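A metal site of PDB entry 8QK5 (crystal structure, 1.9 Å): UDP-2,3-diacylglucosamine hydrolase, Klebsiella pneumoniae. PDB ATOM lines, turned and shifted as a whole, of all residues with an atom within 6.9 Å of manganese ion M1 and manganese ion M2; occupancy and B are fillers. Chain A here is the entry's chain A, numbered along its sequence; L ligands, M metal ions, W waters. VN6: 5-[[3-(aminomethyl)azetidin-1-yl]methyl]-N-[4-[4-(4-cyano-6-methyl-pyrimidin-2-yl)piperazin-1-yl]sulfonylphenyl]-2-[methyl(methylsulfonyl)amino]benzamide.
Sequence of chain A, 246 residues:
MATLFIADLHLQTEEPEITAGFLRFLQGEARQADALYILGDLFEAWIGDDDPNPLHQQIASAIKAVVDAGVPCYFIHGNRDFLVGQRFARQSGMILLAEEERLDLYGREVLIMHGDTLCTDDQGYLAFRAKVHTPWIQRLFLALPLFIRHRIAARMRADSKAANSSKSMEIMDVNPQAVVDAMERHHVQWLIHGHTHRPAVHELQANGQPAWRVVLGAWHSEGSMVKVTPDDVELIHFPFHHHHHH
Manganese ion M1 is bound by OD1 of Asn 79 (2.1 Å), water W1 (2.2 Å), OD2 of Asp 41 (2.2 Å), NE2 of His 114 (2.3 Å) and ND1 of His 195 (2.3 Å).
NH1 of Arg 80 lies within hydrogen-bond range of O36 of the ligand, at 2.7 Å.
The side-chain amide nitrogen (ND2) of Asn 79 lies within hydrogen-bond range of an oxygen (O24) of the ligand (2.8 Å).
Water W1 binds manganese ion M2 (2.1 Å).
The side-chain carboxylate (OD1) of Asp 8 binds manganese ion M2, 2.1 Å away.
OD2 of Asp 41 is bound to manganese ion M2 (2.2 Å).
Manganese ion M2 is bound by NE2 of His 197 (2.2 Å).
A ring nitrogen (NE2) of His 10 binds manganese ion M2 (2.2 Å).
ND1 of His 10 lies within hydrogen-bond range of OE1 of Glu 44 (2.9 Å).
O of Asp 41 lies within hydrogen-bond range of N of Leu 9 (2.9 Å).
The backbone carbonyl oxygen of His 195 lies close to a ring nitrogen (NE2) of His 197, at 3.5 Å.
N of Arg 80 sits at hydrogen-bond distance from OD1 of Asp 41, at 3.1 Å.
The backbone carbonyl oxygen of Gly 40 lies within hydrogen-bond range of the backbone NH of Asp 8, at 2.9 Å.
ND1 of His 114 lies within hydrogen-bond range of O of Leu 39, at 2.7 Å.
The backbone NH (N) of Gly 194 sits at hydrogen-bond distance from the backbone carbonyl oxygen (O) of His 114 (2.7 Å).
The side-chain carboxylate of Asp 8 sits at hydrogen-bond distance from the backbone NH of His 195 (2.7 Å).
The nearest printed residue that does not touch manganese ion M2 is His 195 (4.1 Å).
Of the 20 residues printed, 5 come within 4 Å of manganese ion M1.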
ATOM      1  N   ALA A   7       2.387 -21.615  -3.293  1.00  0.00           N
ATOM      2  CA  ALA A   7       2.768 -20.756  -4.401  1.00  0.00           C
ATOM      3  C   ALA A   7       4.273 -20.897  -4.610  1.00  0.00           C
ATOM      4  O   ALA A   7       4.993 -21.409  -3.754  1.00  0.00           O
ATOM      5  CB  ALA A   7       2.344 -19.339  -4.123  1.00  0.00           C
ATOM      6  N   ASP A   8       4.736 -20.480  -5.792  1.00  0.00           N
ATOM      7  CA  ASP A   8       6.151 -20.243  -5.975  1.00  0.00           C
ATOM      8  C   ASP A   8       6.909 -21.557  -5.864  1.00  0.00           C
ATOM      9  O   ASP A   8       8.024 -21.598  -5.339  1.00  0.00           O
ATOM     10  CB  ASP A   8       6.641 -19.159  -5.009  1.00  0.00           C
ATOM     11  CG  ASP A   8       6.012 -17.810  -5.297  1.00  0.00           C
ATOM     12  OD1 ASP A   8       6.223 -17.288  -6.413  1.00  0.00           O
ATOM     13  OD2 ASP A   8       5.305 -17.281  -4.414  1.00  0.00           O
ATOM     14  N   LEU A   9       6.320 -22.612  -6.426  1.00  0.00           N
ATOM     15  CA  LEU A   9       7.014 -23.881  -6.568  1.00  0.00           C
ATOM     16  C   LEU A   9       8.097 -23.826  -7.664  1.00  0.00           C
ATOM     17  O   LEU A   9       9.091 -24.542  -7.581  1.00  0.00           O
ATOM     18  CB  LEU A   9       5.981 -24.979  -6.850  1.00  0.00           C
ATOM     19  CG  LEU A   9       5.033 -25.261  -5.689  1.00  0.00           C
ATOM     20  CD1 LEU A   9       3.752 -24.478  -5.820  1.00  0.00           C
ATOM     21  CD2 LEU A   9       4.732 -26.730  -5.611  1.00  0.00           C
ATOM     22  N   HIS A  10       7.894 -23.031  -8.715  1.00  0.00           N
ATOM     23  CA  HIS A  10       8.891 -22.914  -9.781  1.00  0.00           C
ATOM     24  C   HIS A  10       9.277 -24.282 -10.359  1.00  0.00           C
ATOM     25  O   HIS A  10      10.455 -24.574 -10.575  1.00  0.00           O
ATOM     26  CB  HIS A  10      10.103 -22.110  -9.283  1.00  0.00           C
ATOM     27  CG  HIS A  10       9.721 -20.714  -8.923  1.00  0.00           C
ATOM     28  ND1 HIS A  10       9.516 -19.781  -9.910  1.00  0.00           N
ATOM     29  CD2 HIS A  10       9.422 -20.109  -7.788  1.00  0.00           C
ATOM     30  CE1 HIS A  10       9.114 -18.643  -9.367  1.00  0.00           C
ATOM     31  NE2 HIS A  10       9.027 -18.819  -8.076  1.00  0.00           N
ATOM     32  N   LEU A  39      -1.281 -20.247  -5.672  1.00  0.00           N
ATOM     33  CA  LEU A  39      -1.324 -18.827  -5.981  1.00  0.00           C
ATOM     34  C   LEU A  39      -0.148 -18.417  -6.869  1.00  0.00           C
ATOM     35  O   LEU A  39       0.515 -17.426  -6.596  1.00  0.00           O
ATOM     36  CB  LEU A  39      -1.315 -18.050  -4.669  1.00  0.00           C
ATOM     37  CG  LEU A  39      -2.361 -18.489  -3.662  1.00  0.00           C
ATOM     38  CD1 LEU A  39      -2.372 -17.495  -2.504  1.00  0.00           C
ATOM     39  CD2 LEU A  39      -3.737 -18.598  -4.301  1.00  0.00           C
ATOM     40  N   GLY A  40       0.088 -19.197  -7.943  1.00  0.00           N
ATOM     41  CA  GLY A  40       0.946 -18.777  -9.041  1.00  0.00           C
ATOM     42  C   GLY A  40       2.377 -19.279  -8.894  1.00  0.00           C
ATOM     43  O   GLY A  40       2.794 -19.718  -7.815  1.00  0.00           O
ATOM     44  N   ASP A  41       3.108 -19.224  -9.997  1.00  0.00           N
ATOM     45  CA  ASP A  41       4.464 -19.709 -10.084  1.00  0.00           C
ATOM     46  C   ASP A  41       4.484 -21.179  -9.688  1.00  0.00           C
ATOM     47  O   ASP A  41       5.417 -21.650  -9.013  1.00  0.00           O
ATOM     48  CB  ASP A  41       5.444 -18.840  -9.294  1.00  0.00           C
ATOM     49  CG  ASP A  41       5.713 -17.503  -9.952  1.00  0.00           C
ATOM     50  OD1 ASP A  41       5.024 -17.214 -10.968  1.00  0.00           O
ATOM     51  OD2 ASP A  41       6.567 -16.740  -9.444  1.00  0.00           O
ATOM     52  N   GLU A  44       8.281 -22.732 -13.372  1.00  0.00           N
ATOM     53  CA  GLU A  44       9.353 -21.765 -13.549  1.00  0.00           C
ATOM     54  C   GLU A  44       9.143 -20.963 -14.821  1.00  0.00           C
ATOM     55  O   GLU A  44       9.594 -19.830 -14.917  1.00  0.00           O
ATOM     56  CB  GLU A  44      10.699 -22.495 -13.586  1.00  0.00           C
ATOM     57  CG  GLU A  44      11.916 -21.626 -13.875  1.00  0.00           C
ATOM     58  CD  GLU A  44      12.137 -20.357 -13.062  1.00  0.00           C
ATOM     59  OE1 GLU A  44      11.421 -20.118 -12.061  1.00  0.00           O
ATOM     60  OE2 GLU A  44      13.012 -19.583 -13.441  1.00  0.00           O
ATOM     61  N   GLY A  78       0.924 -16.680 -11.666  1.00  0.00           N
ATOM     62  CA  GLY A  78       2.015 -15.820 -11.278  1.00  0.00           C
ATOM     63  C   GLY A  78       2.656 -15.124 -12.482  1.00  0.00           C
ATOM     64  O   GLY A  78       2.106 -15.106 -13.577  1.00  0.00           O
ATOM     65  N   ASN A  79       3.790 -14.498 -12.238  1.00  0.00           N
ATOM     66  CA  ASN A  79       4.495 -13.730 -13.247  1.00  0.00           C
ATOM     67  C   ASN A  79       5.209 -14.688 -14.181  1.00  0.00           C
ATOM     68  O   ASN A  79       5.510 -14.320 -15.304  1.00  0.00           O
ATOM     69  CB  ASN A  79       5.476 -12.735 -12.634  1.00  0.00           C
ATOM     70  CG  ASN A  79       6.578 -13.404 -11.832  1.00  0.00           C
ATOM     71  OD1 ASN A  79       6.278 -13.971 -10.806  1.00  0.00           O
ATOM     72  ND2 ASN A  79       7.821 -13.379 -12.272  1.00  0.00           N
ATOM     73  N   ARG A  80       5.474 -15.913 -13.703  1.00  0.00           N
ATOM     74  CA  ARG A  80       6.238 -16.882 -14.477  1.00  0.00           C
ATOM     75  C   ARG A  80       5.317 -17.669 -15.406  1.00  0.00           C
ATOM     76  O   ARG A  80       5.766 -18.055 -16.485  1.00  0.00           O
ATOM     77  CB  ARG A  80       7.043 -17.867 -13.624  1.00  0.00           C
ATOM     78  CG  ARG A  80       8.063 -17.237 -12.664  1.00  0.00           C
ATOM     79  CD  ARG A  80       9.135 -16.405 -13.319  1.00  0.00           C
ATOM     80  NE  ARG A  80       9.939 -17.200 -14.235  1.00  0.00           N
ATOM     81  CZ  ARG A  80      10.956 -16.730 -14.944  1.00  0.00           C
ATOM     82  NH1 ARG A  80      11.338 -15.475 -14.827  1.00  0.00           N
ATOM     83  NH2 ARG A  80      11.579 -17.529 -15.793  1.00  0.00           N
ATOM     84  N   HIS A 114      -1.520 -13.619  -6.356  1.00  0.00           N
ATOM     85  CA  HIS A 114      -0.117 -13.990  -6.517  1.00  0.00           C
ATOM     86  C   HIS A 114       0.744 -13.027  -5.712  1.00  0.00           C
ATOM     87  O   HIS A 114       1.631 -13.457  -4.997  1.00  0.00           O
ATOM     88  CB  HIS A 114       0.334 -13.992  -7.980  1.00  0.00           C
ATOM     89  CG  HIS A 114       1.767 -14.397  -8.097  1.00  0.00           C
ATOM     90  ND1 HIS A 114       2.179 -15.612  -7.597  1.00  0.00           N
ATOM     91  CD2 HIS A 114       2.864 -13.810  -8.628  1.00  0.00           C
ATOM     92  CE1 HIS A 114       3.481 -15.749  -7.855  1.00  0.00           C
ATOM     93  NE2 HIS A 114       3.926 -14.674  -8.482  1.00  0.00           N
ATOM     94  N   ASP A 116       2.266 -10.134  -7.229  1.00  0.00           N
ATOM     95  CA  ASP A 116       3.077  -9.298  -8.102  1.00  0.00           C
ATOM     96  C   ASP A 116       2.411  -7.935  -8.322  1.00  0.00           C
ATOM     97  O   ASP A 116       3.103  -6.927  -8.500  1.00  0.00           O
ATOM     98  CB  ASP A 116       3.374 -10.025  -9.402  1.00  0.00           C
ATOM     99  CG  ASP A 116       2.153 -10.351 -10.257  1.00  0.00           C
ATOM    100  OD1 ASP A 116       1.170 -10.942  -9.737  1.00  0.00           O
ATOM    101  OD2 ASP A 116       2.219 -10.053 -11.451  1.00  0.00           O
ATOM    102  N   TYR A 125       8.909  -4.172 -14.020  1.00  0.00           N
ATOM    103  CA  TYR A 125       8.109  -5.372 -14.056  1.00  0.00           C
ATOM    104  C   TYR A 125       6.682  -5.043 -14.504  1.00  0.00           C
ATOM    105  O   TYR A 125       6.075  -5.834 -15.217  1.00  0.00           O
ATOM    106  CB  TYR A 125       8.090  -6.098 -12.710  1.00  0.00           C
ATOM    107  CG  TYR A 125       7.066  -7.196 -12.721  1.00  0.00           C
ATOM    108  CD1 TYR A 125       7.239  -8.315 -13.521  1.00  0.00           C
ATOM    109  CD2 TYR A 125       5.866  -7.057 -12.061  1.00  0.00           C
ATOM    110  CE1 TYR A 125       6.279  -9.307 -13.619  1.00  0.00           C
ATOM    111  CE2 TYR A 125       4.884  -8.028 -12.145  1.00  0.00           C
ATOM    112  CZ  TYR A 125       5.093  -9.155 -12.935  1.00  0.00           C
ATOM    113  OH  TYR A 125       4.116 -10.107 -13.046  1.00  0.00           O
ATOM    114  N   ILE A 171      13.610 -10.198  -6.186  1.00  0.00           N
ATOM    115  CA  ILE A 171      12.234  -9.871  -6.509  1.00  0.00           C
ATOM    116  C   ILE A 171      11.809  -8.678  -5.631  1.00  0.00           C
ATOM    117  O   ILE A 171      11.944  -8.717  -4.402  1.00  0.00           O
ATOM    118  CB  ILE A 171      11.351 -11.132  -6.379  1.00  0.00           C
ATOM    119  CG1 ILE A 171      11.851 -12.223  -7.336  1.00  0.00           C
ATOM    120  CG2 ILE A 171       9.877 -10.819  -6.584  1.00  0.00           C
ATOM    121  CD1 ILE A 171      10.991 -13.448  -7.422  1.00  0.00           C
ATOM    122  N   GLY A 194       1.929 -14.712  -2.602  1.00  0.00           N
ATOM    123  CA  GLY A 194       3.252 -15.273  -2.782  1.00  0.00           C
ATOM    124  C   GLY A 194       4.124 -14.234  -3.446  1.00  0.00           C
ATOM    125  O   GLY A 194       4.170 -13.076  -3.034  1.00  0.00           O
ATOM    126  N   HIS A 195       4.725 -14.653  -4.561  1.00  0.00           N
ATOM    127  CA  HIS A 195       5.499 -13.802  -5.451  1.00  0.00           C
ATOM    128  C   HIS A 195       6.835 -13.338  -4.853  1.00  0.00           C
ATOM    129  O   HIS A 195       7.866 -13.442  -5.515  1.00  0.00           O
ATOM    130  CB  HIS A 195       4.711 -12.590  -5.927  1.00  0.00           C
ATOM    131  CG  HIS A 195       5.539 -11.853  -6.932  1.00  0.00           C
ATOM    132  ND1 HIS A 195       6.040 -12.438  -8.081  1.00  0.00           N
ATOM    133  CD2 HIS A 195       6.055 -10.616  -6.859  1.00  0.00           C
ATOM    134  CE1 HIS A 195       6.730 -11.511  -8.741  1.00  0.00           C
ATOM    135  NE2 HIS A 195       6.783 -10.415  -8.005  1.00  0.00           N
ATOM    136  N   THR A 196       6.817 -12.796  -3.636  1.00  0.00           N
ATOM    137  CA  THR A 196       7.992 -12.156  -3.073  1.00  0.00           C
ATOM    138  C   THR A 196       9.048 -13.120  -2.534  1.00  0.00           C
ATOM    139  O   THR A 196      10.175 -12.683  -2.273  1.00  0.00           O
ATOM    140  CB  THR A 196       7.637 -11.166  -1.957  1.00  0.00           C
ATOM    141  OG1 THR A 196       7.007 -11.871  -0.894  1.00  0.00           O
ATOM    142  CG2 THR A 196       6.738 -10.034  -2.406  1.00  0.00           C
ATOM    143  N   HIS A 197       8.678 -14.381  -2.288  1.00  0.00           N
ATOM    144  CA  HIS A 197       9.580 -15.397  -1.739  1.00  0.00           C
ATOM    145  C   HIS A 197      10.146 -14.979  -0.376  1.00  0.00           C
ATOM    146  O   HIS A 197      11.243 -15.405  -0.024  1.00  0.00           O
ATOM    147  CB  HIS A 197      10.732 -15.692  -2.698  1.00  0.00           C
ATOM    148  CG  HIS A 197      10.305 -16.072  -4.081  1.00  0.00           C
ATOM    149  ND1 HIS A 197      11.208 -16.228  -5.114  1.00  0.00           N
ATOM    150  CD2 HIS A 197       9.089 -16.306  -4.604  1.00  0.00           C
ATOM    151  CE1 HIS A 197      10.544 -16.522  -6.224  1.00  0.00           C
ATOM    152  NE2 HIS A 197       9.262 -16.586  -5.940  1.00  0.00           N
ATOM    153  N   ALA A 218       8.932 -19.614  -1.510  1.00  0.00           N
ATOM    154  CA  ALA A 218       9.302 -20.427  -2.657  1.00  0.00           C
ATOM    155  C   ALA A 218       9.754 -21.817  -2.211  1.00  0.00           C
ATOM    156  O   ALA A 218      10.284 -21.968  -1.112  1.00  0.00           O
ATOM    157  CB  ALA A 218      10.379 -19.738  -3.468  1.00  0.00           C
HETATM  158  C5  VN6 L   1       4.355 -13.304 -24.379  1.00  0.00           C
HETATM  159  C6  VN6 L   1       5.139 -12.602 -25.263  1.00  0.00           C
HETATM  160  N7  VN6 L   1       6.887 -15.201 -22.652  1.00  0.00           N
HETATM  161  C8  VN6 L   1       6.002 -16.160 -21.993  1.00  0.00           C
HETATM  162  C26 VN6 L   1      10.287  -9.478 -15.772  1.00  0.00           C
HETATM  163  C27 VN6 L   1      10.845  -8.274 -15.312  1.00  0.00           C
HETATM  164  C28 VN6 L   1      11.168  -8.124 -13.967  1.00  0.00           C
HETATM  165  C29 VN6 L   1      10.945  -9.158 -13.066  1.00  0.00           C
HETATM  166  C30 VN6 L   1      10.418 -10.365 -13.494  1.00  0.00           C
HETATM  167  C32 VN6 L   1       9.938 -10.826 -11.170  1.00  0.00           C
HETATM  168  C37 VN6 L   1       2.834 -13.107 -24.326  1.00  0.00           C
HETATM  169  C38 VN6 L   1       7.349 -12.071 -26.145  1.00  0.00           C
HETATM  170  C40 VN6 L   1      11.072  -7.099 -16.205  1.00  0.00           C
HETATM  171  C42 VN6 L   1      12.088  -6.068 -18.057  1.00  0.00           C
HETATM  172  C1  VN6 L   1       6.507 -12.790 -25.261  1.00  0.00           C
HETATM  173  N2  VN6 L   1       7.056 -13.663 -24.421  1.00  0.00           N
HETATM  174  C3  VN6 L   1       6.278 -14.407 -23.610  1.00  0.00           C
HETATM  175  N4  VN6 L   1       4.941 -14.183 -23.543  1.00  0.00           N
HETATM  176  C9  VN6 L   1       6.651 -16.454 -20.640  1.00  0.00           C
HETATM  177  C10 VN6 L   1       8.115 -15.785 -23.043  1.00  0.00           C
HETATM  178  C11 VN6 L   1       8.876 -16.122 -21.738  1.00  0.00           C
HETATM  179  N12 VN6 L   1       8.015 -17.020 -20.866  1.00  0.00           N
HETATM  180  S13 VN6 L   1       8.767 -17.401 -19.429  1.00  0.00           S
HETATM  181  C14 VN6 L   1       9.104 -15.950 -18.515  1.00  0.00           C
HETATM  182  O15 VN6 L   1       7.905 -18.281 -18.699  1.00  0.00           O
HETATM  183  O16 VN6 L   1       9.993 -18.049 -19.752  1.00  0.00           O
HETATM  184  C17 VN6 L   1      10.308 -15.335 -18.691  1.00  0.00           C
HETATM  185  C18 VN6 L   1      10.610 -14.192 -17.997  1.00  0.00           C
HETATM  186  C19 VN6 L   1       9.707 -13.617 -17.111  1.00  0.00           C
HETATM  187  C20 VN6 L   1       8.138 -15.380 -17.628  1.00  0.00           C
HETATM  188  C21 VN6 L   1       8.462 -14.188 -16.937  1.00  0.00           C
HETATM  189  N22 VN6 L   1      10.066 -12.401 -16.507  1.00  0.00           N
HETATM  190  C23 VN6 L   1       9.478 -11.860 -15.391  1.00  0.00           C
HETATM  191  O24 VN6 L   1       8.534 -12.428 -14.830  1.00  0.00           O
HETATM  192  C25 VN6 L   1      10.043 -10.515 -14.866  1.00  0.00           C
HETATM  193  N31 VN6 L   1      10.140 -11.417 -12.536  1.00  0.00           N
HETATM  194  S33 VN6 L   1      11.342 -12.519 -12.495  1.00  0.00           S
HETATM  195  C34 VN6 L   1      12.822 -11.778 -11.824  1.00  0.00           C
HETATM  196  O35 VN6 L   1      10.902 -13.610 -11.684  1.00  0.00           O
HETATM  197  O36 VN6 L   1      11.603 -13.008 -13.820  1.00  0.00           O
HETATM  198  N39 VN6 L   1       8.036 -11.507 -26.833  1.00  0.00           N
HETATM  199  N41 VN6 L   1      11.892  -7.382 -17.354  1.00  0.00           N
HETATM  200  C43 VN6 L   1      13.332  -7.419 -16.980  1.00  0.00           C
HETATM  201  C44 VN6 L   1      13.591  -6.329 -18.009  1.00  0.00           C
HETATM  202  C45 VN6 L   1      14.009  -6.972 -19.334  1.00  0.00           C
HETATM  203  N46 VN6 L   1      14.991  -6.125 -20.032  1.00  0.00           N
HETATM  204 MN    MN M   1       6.195 -14.648  -8.788  1.00  0.00          MN
HETATM  205 MN    MN M   2       7.906 -16.922  -7.686  1.00  0.00          MN
HETATM  206  O   HOH W   1       8.189 -14.812  -7.830  1.00  0.00           O
